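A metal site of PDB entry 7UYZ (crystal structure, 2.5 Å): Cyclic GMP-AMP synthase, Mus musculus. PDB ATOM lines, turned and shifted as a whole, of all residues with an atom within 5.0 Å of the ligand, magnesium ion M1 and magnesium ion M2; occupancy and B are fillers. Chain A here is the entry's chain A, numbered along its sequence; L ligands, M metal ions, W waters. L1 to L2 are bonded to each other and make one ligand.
The backbone NH (N) of Ser 56 sits close to an oxygen (O5) of LG2 L2. OG of Ser 56 lies within hydrogen-bond range of O4 of LG2 L2 (2.5 Å). O7 of LIG L1 is in hydrogen-bond range of N of Ser 277 (2.7 Å). OG of Ser 277 lies within hydrogen-bond range of O3 of LG2 L2. NZ of Lys 145 lies within hydrogen-bond range of O5 of LIG L1, at 2.7 Å. The side-chain amino group of Lys 259 is in salt-bridge range of an oxygen (O1) of LG2 L2 (2.8 Å). The side-chain sulfur of Cys 276 is in hydrogen-bond range of an oxygen (O11) of LG2 L2, at 3.1 Å.
The side-chain hydroxyl (OG) of Ser 56 lies within hydrogen-bond range of the side-chain amino group (NZ) of Lys 259 (3.2 Å). The backbone carbonyl oxygen (O) of Ser 56 lies within hydrogen-bond range of the backbone NH (N) of Lys 62, at 3.3 Å. The side-chain sulfur (SG) of Cys 276 lies close to the backbone NH (N) of Tyr 278 (3.7 Å). NE2 of His 324 lies close to OH of Tyr 278 (3.3 Å). O of Phe 275 sits at hydrogen-bond distance from NZ of Lys 266, at 2.8 Å.
Gly 55 touches the ligand. Lys 62 touches the ligand. O of Gly 147 touches O2 of LIG L1 (3.997 Å). NZ of Lys 266 touches N2 of LIG L1 (3.8 Å). Phe 275 touches the ligand. CE2 of Tyr 278 touches O14 of LG2 L2, at 3.5 Å. 13 residues have an atom within 4 Å of the ligand: Gly 55, Ser 56, Lys 62, Glu 68, Asp 70, Lys 145, Gly 147, Lys 259, Lys 266, Phe 275, Cys 276, Ser 277 and Tyr 278.
Three residues have an atom within 4 Å of magnesium ion M1: Glu 68, Asp 70 and Asp 164. The nearest printed residue that does not touch magnesium ion M1 is Ser 277 (7.2 Å).
Within 4 Å of magnesium ion M2: Glu 68 and Asp 70.
Magnesium ion M1 is bound by OE2 of Glu 68, OD2 of Asp 164, O8 of LG2 L2 and OD1 of Asp 70. Magnesium ion M1 has four donor atoms within binding distance.
Magnesium ion M2 is bound by water W1 (2.1 Å), O2 of LG2 L2 (2.1 Å), OE1 of Glu 68 (2.2 Å), OD2 of Asp 70 (2.2 Å), O5 of LG2 L2 (2.2 Å) and O8 of LG2 L2 (2.3 Å).
Water W1 lies within hydrogen-bond range of O of Glu 68 (3.2 Å) and OG of Ser 56 (3.4 Å). Water W2 lies within hydrogen-bond range of OE1 of Glu 59 (2.5 Å), O6 of LG2 L2 (2.7 Å) and OG of Ser 56 (3.5 Å). Water W7 lies within hydrogen-bond range of an oxygen (O6) of LG2 L2, the side-chain hydroxyl of Ser 277 and the backbone NH of Tyr 278. Water W3 lies within hydrogen-bond range of OE2 of Glu 263 (2.6 Å), O3 of LG2 L2 (3.3 Å) and NZ of Lys 259 (3.3 Å). Water W4 bridges the side-chain hydroxyl (OG) of Ser 148 and an oxygen (O12) of LG2 L2. Water W5 lies within hydrogen-bond range of NH2 of Arg 221 and N5 of LG2 L2.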
ATOM      1  N   GLY A  55     -27.936  18.679 -34.614  1.00  0.00           N
ATOM      2  CA  GLY A  55     -28.324  19.598 -33.555  1.00  0.00           C
ATOM      3  C   GLY A  55     -29.794  19.491 -33.189  1.00  0.00           C
ATOM      4  O   GLY A  55     -30.518  18.637 -33.709  1.00  0.00           O
ATOM      5  N   SER A  56     -30.219  20.417 -32.313  1.00  0.00           N
ATOM      6  CA  SER A  56     -31.531  20.443 -31.684  1.00  0.00           C
ATOM      7  C   SER A  56     -32.676  20.221 -32.624  1.00  0.00           C
ATOM      8  O   SER A  56     -33.577  19.436 -32.335  1.00  0.00           O
ATOM      9  CB  SER A  56     -31.803  21.804 -31.057  1.00  0.00           C
ATOM     10  OG  SER A  56     -30.801  22.123 -30.158  1.00  0.00           O
ATOM     11  N   GLU A  59     -32.883  16.914 -33.966  1.00  0.00           N
ATOM     12  CA  GLU A  59     -33.091  16.018 -32.823  1.00  0.00           C
ATOM     13  C   GLU A  59     -34.485  16.142 -32.150  1.00  0.00           C
ATOM     14  O   GLU A  59     -34.802  15.377 -31.250  1.00  0.00           O
ATOM     15  CB  GLU A  59     -32.002  16.252 -31.785  1.00  0.00           C
ATOM     16  CG  GLU A  59     -30.628  15.709 -32.178  1.00  0.00           C
ATOM     17  CD  GLU A  59     -29.514  16.269 -31.299  1.00  0.00           C
ATOM     18  OE1 GLU A  59     -29.812  17.145 -30.450  1.00  0.00           O
ATOM     19  OE2 GLU A  59     -28.353  15.832 -31.451  1.00  0.00           O
ATOM     20  N   LYS A  62     -35.241  21.340 -30.152  1.00  0.00           N
ATOM     21  CA  LYS A  62     -35.159  22.791 -30.305  1.00  0.00           C
ATOM     22  C   LYS A  62     -36.328  23.377 -29.542  1.00  0.00           C
ATOM     23  O   LYS A  62     -37.439  22.897 -29.648  1.00  0.00           O
ATOM     24  CB  LYS A  62     -35.211  23.199 -31.770  1.00  0.00           C
ATOM     25  CG  LYS A  62     -34.998  24.706 -32.009  1.00  0.00           C
ATOM     26  CD  LYS A  62     -33.541  25.108 -31.809  1.00  0.00           C
ATOM     27  CE  LYS A  62     -33.345  26.610 -31.967  1.00  0.00           C
ATOM     28  NZ  LYS A  62     -34.163  27.428 -31.058  1.00  0.00           N
ATOM     29  N   GLU A  68     -32.508  28.503 -35.009  1.00  0.00           N
ATOM     30  CA  GLU A  68     -31.128  28.091 -35.076  1.00  0.00           C
ATOM     31  C   GLU A  68     -31.081  26.672 -35.617  1.00  0.00           C
ATOM     32  O   GLU A  68     -31.769  25.783 -35.122  1.00  0.00           O
ATOM     33  CB  GLU A  68     -30.445  28.257 -33.714  1.00  0.00           C
ATOM     34  CG  GLU A  68     -28.932  28.487 -33.773  1.00  0.00           C
ATOM     35  CD  GLU A  68     -28.112  27.197 -33.730  1.00  0.00           C
ATOM     36  OE1 GLU A  68     -28.726  26.120 -33.633  1.00  0.00           O
ATOM     37  OE2 GLU A  68     -26.859  27.250 -33.783  1.00  0.00           O
ATOM     38  N   ASP A  70     -28.328  23.671 -37.477  1.00  0.00           N
ATOM     39  CA  ASP A  70     -26.950  23.236 -37.638  1.00  0.00           C
ATOM     40  C   ASP A  70     -26.844  22.217 -38.768  1.00  0.00           C
ATOM     41  O   ASP A  70     -27.602  21.236 -38.800  1.00  0.00           O
ATOM     42  CB  ASP A  70     -26.418  22.690 -36.316  1.00  0.00           C
ATOM     43  CG  ASP A  70     -26.692  23.650 -35.164  1.00  0.00           C
ATOM     44  OD1 ASP A  70     -25.929  24.644 -34.993  1.00  0.00           O
ATOM     45  OD2 ASP A  70     -27.692  23.415 -34.453  1.00  0.00           O
ATOM     46  N   GLU A 142     -22.346  36.094 -40.783  1.00  0.00           N
ATOM     47  CA  GLU A 142     -21.972  36.701 -39.517  1.00  0.00           C
ATOM     48  C   GLU A 142     -20.456  36.816 -39.481  1.00  0.00           C
ATOM     49  O   GLU A 142     -19.747  36.003 -40.050  1.00  0.00           O
ATOM     50  CB  GLU A 142     -22.489  35.845 -38.357  1.00  0.00           C
ATOM     51  CG  GLU A 142     -22.443  36.443 -36.956  1.00  0.00           C
ATOM     52  CD  GLU A 142     -22.754  35.383 -35.867  1.00  0.00           C
ATOM     53  OE1 GLU A 142     -21.884  34.527 -35.586  1.00  0.00           O
ATOM     54  OE2 GLU A 142     -23.882  35.357 -35.327  1.00  0.00           O
ATOM     55  N   LYS A 145     -16.462  34.418 -35.386  1.00  0.00           N
ATOM     56  CA  LYS A 145     -16.207  34.347 -33.973  1.00  0.00           C
ATOM     57  C   LYS A 145     -15.052  33.368 -33.768  1.00  0.00           C
ATOM     58  O   LYS A 145     -15.112  32.251 -34.266  1.00  0.00           O
ATOM     59  CB  LYS A 145     -17.437  33.850 -33.234  1.00  0.00           C
ATOM     60  CG  LYS A 145     -18.525  34.896 -33.229  1.00  0.00           C
ATOM     61  CD  LYS A 145     -19.709  34.459 -32.392  1.00  0.00           C
ATOM     62  CE  LYS A 145     -20.729  35.593 -32.330  1.00  0.00           C
ATOM     63  NZ  LYS A 145     -21.712  35.367 -31.231  1.00  0.00           N
ATOM     64  N   GLY A 147     -12.700  30.553 -32.037  1.00  0.00           N
ATOM     65  CA  GLY A 147     -13.113  29.348 -31.353  1.00  0.00           C
ATOM     66  C   GLY A 147     -14.229  28.619 -32.048  1.00  0.00           C
ATOM     67  O   GLY A 147     -14.647  27.571 -31.553  1.00  0.00           O
ATOM     68  N   SER A 148     -14.730  29.134 -33.182  1.00  0.00           N
ATOM     69  CA  SER A 148     -15.842  28.512 -33.891  1.00  0.00           C
ATOM     70  C   SER A 148     -15.471  27.841 -35.220  1.00  0.00           C
ATOM     71  O   SER A 148     -14.827  28.436 -36.062  1.00  0.00           O
ATOM     72  CB  SER A 148     -16.976  29.498 -34.119  1.00  0.00           C
ATOM     73  OG  SER A 148     -18.079  28.827 -34.720  1.00  0.00           O
ATOM     74  N   ASP A 164     -25.634  27.572 -38.703  1.00  0.00           N
ATOM     75  CA  ASP A 164     -24.226  27.245 -38.610  1.00  0.00           C
ATOM     76  C   ASP A 164     -23.943  26.246 -39.731  1.00  0.00           C
ATOM     77  O   ASP A 164     -24.505  25.144 -39.736  1.00  0.00           O
ATOM     78  CB  ASP A 164     -23.899  26.594 -37.255  1.00  0.00           C
ATOM     79  CG  ASP A 164     -24.030  27.552 -36.081  1.00  0.00           C
ATOM     80  OD1 ASP A 164     -23.872  28.775 -36.268  1.00  0.00           O
ATOM     81  OD2 ASP A 164     -24.316  27.064 -34.954  1.00  0.00           O
ATOM     82  N   ARG A 221     -10.852  19.279 -34.154  1.00  0.00           N
ATOM     83  CA  ARG A 221     -11.576  18.688 -32.982  1.00  0.00           C
ATOM     84  C   ARG A 221     -12.567  17.622 -33.482  1.00  0.00           C
ATOM     85  O   ARG A 221     -13.212  17.875 -34.525  1.00  0.00           O
ATOM     86  CB  ARG A 221     -12.305  19.761 -32.169  1.00  0.00           C
ATOM     87  CG  ARG A 221     -13.062  19.223 -30.947  1.00  0.00           C
ATOM     88  CD  ARG A 221     -13.799  20.292 -30.161  1.00  0.00           C
ATOM     89  NE  ARG A 221     -15.140  20.598 -30.683  1.00  0.00           N
ATOM     90  CZ  ARG A 221     -15.528  21.762 -31.236  1.00  0.00           C
ATOM     91  NH1 ARG A 221     -14.686  22.782 -31.392  1.00  0.00           N
ATOM     92  NH2 ARG A 221     -16.791  21.905 -31.636  1.00  0.00           N
ATOM     93  N   SER A 225     -21.756  14.471 -33.647  1.00  0.00           N
ATOM     94  CA  SER A 225     -23.093  14.972 -33.813  1.00  0.00           C
ATOM     95  C   SER A 225     -24.023  14.000 -34.494  1.00  0.00           C
ATOM     96  O   SER A 225     -25.221  14.011 -34.227  1.00  0.00           O
ATOM     97  CB  SER A 225     -23.089  16.231 -34.658  1.00  0.00           C
ATOM     98  OG  SER A 225     -22.478  17.259 -33.950  1.00  0.00           O
ATOM     99  N   LYS A 259     -32.218  22.861 -20.929  1.00  0.00           N
ATOM    100  CA  LYS A 259     -31.778  23.744 -21.987  1.00  0.00           C
ATOM    101  C   LYS A 259     -32.350  25.144 -21.807  1.00  0.00           C
ATOM    102  O   LYS A 259     -31.641  26.138 -22.007  1.00  0.00           O
ATOM    103  CB  LYS A 259     -32.224  23.206 -23.364  1.00  0.00           C
ATOM    104  CG  LYS A 259     -31.253  22.242 -23.991  1.00  0.00           C
ATOM    105  CD  LYS A 259     -31.935  21.410 -25.057  1.00  0.00           C
ATOM    106  CE  LYS A 259     -32.213  22.216 -26.319  1.00  0.00           C
ATOM    107  NZ  LYS A 259     -30.959  22.658 -27.000  1.00  0.00           N
ATOM    108  N   GLU A 263     -30.436  28.726 -21.173  1.00  0.00           N
ATOM    109  CA  GLU A 263     -30.720  29.818 -22.123  1.00  0.00           C
ATOM    110  C   GLU A 263     -31.233  31.084 -21.424  1.00  0.00           C
ATOM    111  O   GLU A 263     -30.816  32.217 -21.750  1.00  0.00           O
ATOM    112  CB  GLU A 263     -31.747  29.383 -23.187  1.00  0.00           C
ATOM    113  CG  GLU A 263     -31.191  28.566 -24.341  1.00  0.00           C
ATOM    114  CD  GLU A 263     -32.190  28.332 -25.460  1.00  0.00           C
ATOM    115  OE1 GLU A 263     -33.033  29.230 -25.688  1.00  0.00           O
ATOM    116  OE2 GLU A 263     -32.145  27.261 -26.124  1.00  0.00           O
ATOM    117  N   LYS A 266     -28.471  32.555 -19.270  1.00  0.00           N
ATOM    118  CA  LYS A 266     -27.418  33.052 -20.148  1.00  0.00           C
ATOM    119  C   LYS A 266     -27.787  34.403 -20.751  1.00  0.00           C
ATOM    120  O   LYS A 266     -26.931  35.280 -20.902  1.00  0.00           O
ATOM    121  CB  LYS A 266     -27.137  32.073 -21.300  1.00  0.00           C
ATOM    122  CG  LYS A 266     -26.559  30.721 -20.913  1.00  0.00           C
ATOM    123  CD  LYS A 266     -25.130  30.526 -21.335  1.00  0.00           C
ATOM    124  CE  LYS A 266     -24.934  30.491 -22.856  1.00  0.00           C
ATOM    125  NZ  LYS A 266     -23.629  31.156 -23.064  1.00  0.00           N
ATOM    126  N   PHE A 275     -20.522  28.858 -20.507  1.00  0.00           N
ATOM    127  CA  PHE A 275     -21.426  27.740 -20.573  1.00  0.00           C
ATOM    128  C   PHE A 275     -22.222  27.694 -21.868  1.00  0.00           C
ATOM    129  O   PHE A 275     -22.429  28.709 -22.505  1.00  0.00           O
ATOM    130  CB  PHE A 275     -22.374  27.792 -19.391  1.00  0.00           C
ATOM    131  CG  PHE A 275     -21.683  27.695 -18.090  1.00  0.00           C
ATOM    132  CD1 PHE A 275     -21.210  26.464 -17.654  1.00  0.00           C
ATOM    133  CD2 PHE A 275     -21.470  28.815 -17.320  1.00  0.00           C
ATOM    134  CE1 PHE A 275     -20.537  26.360 -16.452  1.00  0.00           C
ATOM    135  CE2 PHE A 275     -20.792  28.723 -16.113  1.00  0.00           C
ATOM    136  CZ  PHE A 275     -20.337  27.476 -15.677  1.00  0.00           C
ATOM    137  N   CYS A 276     -22.670  26.492 -22.249  1.00  0.00           N
ATOM    138  CA  CYS A 276     -23.356  26.283 -23.507  1.00  0.00           C
ATOM    139  C   CYS A 276     -24.247  25.065 -23.394  1.00  0.00           C
ATOM    140  O   CYS A 276     -24.048  24.249 -22.517  1.00  0.00           O
ATOM    141  CB  CYS A 276     -22.361  26.100 -24.644  1.00  0.00           C
ATOM    142  SG  CYS A 276     -21.409  24.571 -24.578  1.00  0.00           S
ATOM    143  N   SER A 277     -25.204  24.942 -24.308  1.00  0.00           N
ATOM    144  CA  SER A 277     -26.170  23.856 -24.299  1.00  0.00           C
ATOM    145  C   SER A 277     -25.510  22.466 -24.358  1.00  0.00           C
ATOM    146  O   SER A 277     -26.090  21.499 -23.903  1.00  0.00           O
ATOM    147  CB  SER A 277     -27.180  24.011 -25.438  1.00  0.00           C
ATOM    148  OG  SER A 277     -26.544  23.890 -26.700  1.00  0.00           O
ATOM    149  N   TYR A 278     -24.315  22.368 -24.941  1.00  0.00           N
ATOM    150  CA  TYR A 278     -23.615  21.077 -25.100  1.00  0.00           C
ATOM    151  C   TYR A 278     -23.258  20.532 -23.715  1.00  0.00           C
ATOM    152  O   TYR A 278     -23.097  19.306 -23.569  1.00  0.00           O
ATOM    153  CB  TYR A 278     -22.367  21.186 -25.993  1.00  0.00           C
ATOM    154  CG  TYR A 278     -21.845  19.820 -26.393  1.00  0.00           C
ATOM    155  CD1 TYR A 278     -22.563  19.039 -27.289  1.00  0.00           C
ATOM    156  CD2 TYR A 278     -20.696  19.266 -25.832  1.00  0.00           C
ATOM    157  CE1 TYR A 278     -22.140  17.776 -27.640  1.00  0.00           C
ATOM    158  CE2 TYR A 278     -20.261  17.997 -26.178  1.00  0.00           C
ATOM    159  CZ  TYR A 278     -20.998  17.241 -27.080  1.00  0.00           C
ATOM    160  OH  TYR A 278     -20.602  15.989 -27.452  1.00  0.00           O
ATOM    161  N   LYS A 281     -26.313  18.806 -22.566  1.00  0.00           N
ATOM    162  CA  LYS A 281     -26.587  17.642 -23.416  1.00  0.00           C
ATOM    163  C   LYS A 281     -25.706  16.493 -22.954  1.00  0.00           C
ATOM    164  O   LYS A 281     -26.152  15.359 -22.866  1.00  0.00           O
ATOM    165  CB  LYS A 281     -26.289  17.973 -24.886  1.00  0.00           C
ATOM    166  CG  LYS A 281     -26.753  16.943 -25.893  1.00  0.00           C
ATOM    167  CD  LYS A 281     -26.321  17.311 -27.306  1.00  0.00           C
ATOM    168  CE  LYS A 281     -27.145  16.598 -28.363  1.00  0.00           C
ATOM    169  NZ  LYS A 281     -26.443  16.490 -29.693  1.00  0.00           N
ATOM    170  N   HIS A 324     -16.602  14.549 -21.383  1.00  0.00           N
ATOM    171  CA  HIS A 324     -17.183  14.335 -22.704  1.00  0.00           C
ATOM    172  C   HIS A 324     -17.678  12.885 -22.756  1.00  0.00           C
ATOM    173  O   HIS A 324     -16.966  11.995 -22.309  1.00  0.00           O
ATOM    174  CB  HIS A 324     -16.124  14.588 -23.763  1.00  0.00           C
ATOM    175  CG  HIS A 324     -16.679  14.850 -25.119  1.00  0.00           C
ATOM    176  ND1 HIS A 324     -17.366  13.891 -25.840  1.00  0.00           N
ATOM    177  CD2 HIS A 324     -16.658  15.957 -25.891  1.00  0.00           C
ATOM    178  CE1 HIS A 324     -17.729  14.402 -27.010  1.00  0.00           C
ATOM    179  NE2 HIS A 324     -17.311  15.655 -27.059  1.00  0.00           N
HETATM  180  P1  LIG L   1     -18.927  27.710 -28.915  1.00  0.00           P
HETATM  181  O1  LIG L   1     -18.583  28.201 -27.537  1.00  0.00           O
HETATM  182  O2  LIG L   1     -18.009  26.706 -29.572  1.00  0.00           O
HETATM  183  O3  LIG L   1     -19.063  28.918 -29.956  1.00  0.00           O
HETATM  184  C1  LIG L   1     -19.432  30.244 -29.503  1.00  0.00           C
HETATM  185  C2  LIG L   1     -20.676  30.689 -30.237  1.00  0.00           C
HETATM  186  O4  LIG L   1     -21.787  29.840 -29.844  1.00  0.00           O
HETATM  187  C3  LIG L   1     -21.148  32.115 -29.950  1.00  0.00           C
HETATM  188  O5  LIG L   1     -21.864  32.660 -31.056  1.00  0.00           O
HETATM  189  C4  LIG L   1     -22.073  31.888 -28.757  1.00  0.00           C
HETATM  190  O6  LIG L   1     -22.962  32.964 -28.543  1.00  0.00           O
HETATM  191  C5  LIG L   1     -22.781  30.615 -29.203  1.00  0.00           C
HETATM  192  N1  LIG L   1     -23.371  29.806 -28.136  1.00  0.00           N
HETATM  193  C6  LIG L   1     -22.977  29.689 -26.822  1.00  0.00           C
HETATM  194  N2  LIG L   1     -23.752  28.887 -26.130  1.00  0.00           N
HETATM  195  C7  LIG L   1     -24.698  28.439 -27.047  1.00  0.00           C
HETATM  196  C8  LIG L   1     -25.788  27.554 -26.873  1.00  0.00           C
HETATM  197  O7  LIG L   1     -26.136  26.958 -25.849  1.00  0.00           O
HETATM  198  N3  LIG L   1     -26.495  27.380 -28.069  1.00  0.00           N
HETATM  199  C9  LIG L   1     -26.200  27.988 -29.272  1.00  0.00           C
HETATM  200  N4  LIG L   1     -26.997  27.709 -30.315  1.00  0.00           N
HETATM  201  N5  LIG L   1     -25.175  28.829 -29.427  1.00  0.00           N
HETATM  202  C10 LIG L   1     -24.476  28.999 -28.281  1.00  0.00           C
HETATM  203  P1  LG2 L   2     -29.216  24.495 -29.359  1.00  0.00           P
HETATM  204  O1  LG2 L   2     -30.707  24.433 -29.118  1.00  0.00           O
HETATM  205  O2  LG2 L   2     -28.890  25.017 -30.740  1.00  0.00           O
HETATM  206  O3  LG2 L   2     -28.470  25.202 -28.260  1.00  0.00           O
HETATM  207  O4  LG2 L   2     -28.640  22.970 -29.323  1.00  0.00           O
HETATM  208  P2  LG2 L   2     -27.608  22.217 -30.278  1.00  0.00           P
HETATM  209  O5  LG2 L   2     -28.120  22.250 -31.672  1.00  0.00           O
HETATM  210  O6  LG2 L   2     -27.203  20.911 -29.662  1.00  0.00           O
HETATM  211  O7  LG2 L   2     -26.372  23.241 -30.193  1.00  0.00           O
HETATM  212  P3  LG2 L   2     -25.388  23.998 -31.207  1.00  0.00           P
HETATM  213  O8  LG2 L   2     -26.161  24.811 -32.207  1.00  0.00           O
HETATM  214  O9  LG2 L   2     -24.363  23.044 -31.717  1.00  0.00           O
HETATM  215  O10 LG2 L   2     -24.664  25.005 -30.182  1.00  0.00           O
HETATM  216  C1  LG2 L   2     -24.094  24.567 -28.914  1.00  0.00           C
HETATM  217  C2  LG2 L   2     -22.851  25.372 -28.650  1.00  0.00           C
HETATM  218  O11 LG2 L   2     -22.068  24.743 -27.614  1.00  0.00           O
HETATM  219  C3  LG2 L   2     -21.888  25.505 -29.829  1.00  0.00           C
HETATM  220  O12 LG2 L   2     -22.276  26.572 -30.698  1.00  0.00           O
HETATM  221  C4  LG2 L   2     -20.567  25.778 -29.122  1.00  0.00           C
HETATM  222  O13 LG2 L   2     -20.444  27.171 -28.863  1.00  0.00           O
HETATM  223  C5  LG2 L   2     -20.691  24.966 -27.838  1.00  0.00           C
HETATM  224  N1  LG2 L   2     -19.989  23.687 -27.893  1.00  0.00           N
HETATM  225  C6  LG2 L   2     -18.857  23.340 -27.196  1.00  0.00           C
HETATM  226  N2  LG2 L   2     -18.433  22.131 -27.448  1.00  0.00           N
HETATM  227  C7  LG2 L   2     -19.342  21.632 -28.378  1.00  0.00           C
HETATM  228  C8  LG2 L   2     -19.406  20.375 -29.022  1.00  0.00           C
HETATM  229  O14 LG2 L   2     -18.634  19.408 -28.883  1.00  0.00           O
HETATM  230  N3  LG2 L   2     -20.495  20.290 -29.891  1.00  0.00           N
HETATM  231  C9  LG2 L   2     -21.407  21.292 -30.102  1.00  0.00           C
HETATM  232  N4  LG2 L   2     -22.400  21.029 -30.965  1.00  0.00           N
HETATM  233  N5  LG2 L   2     -21.353  22.482 -29.506  1.00  0.00           N
HETATM  234  C10 LG2 L   2     -20.307  22.582 -28.655  1.00  0.00           C
HETATM  235 MG    MG M   1     -25.207  26.226 -33.341  1.00  0.00          MG
HETATM  236 MG    MG M   2     -28.392  24.260 -32.593  1.00  0.00          MG
HETATM  237  O   HOH W   1     -30.366  23.853 -33.001  1.00  0.00           O
HETATM  238  O   HOH W   2     -29.244  19.222 -29.114  1.00  0.00           O
HETATM  239  O   HOH W   3     -30.238  25.523 -25.522  1.00  0.00           O
HETATM  240  O   HOH W   4     -20.163  26.885 -33.196  1.00  0.00           O
HETATM  241  O   HOH W   5     -19.200  22.786 -32.187  1.00  0.00           O
HETATM  242  O   HOH W   6     -32.890  25.560 -28.665  1.00  0.00           O
HETATM  243  O   HOH W   7     -26.082  21.154 -27.202  1.00  0.00           O
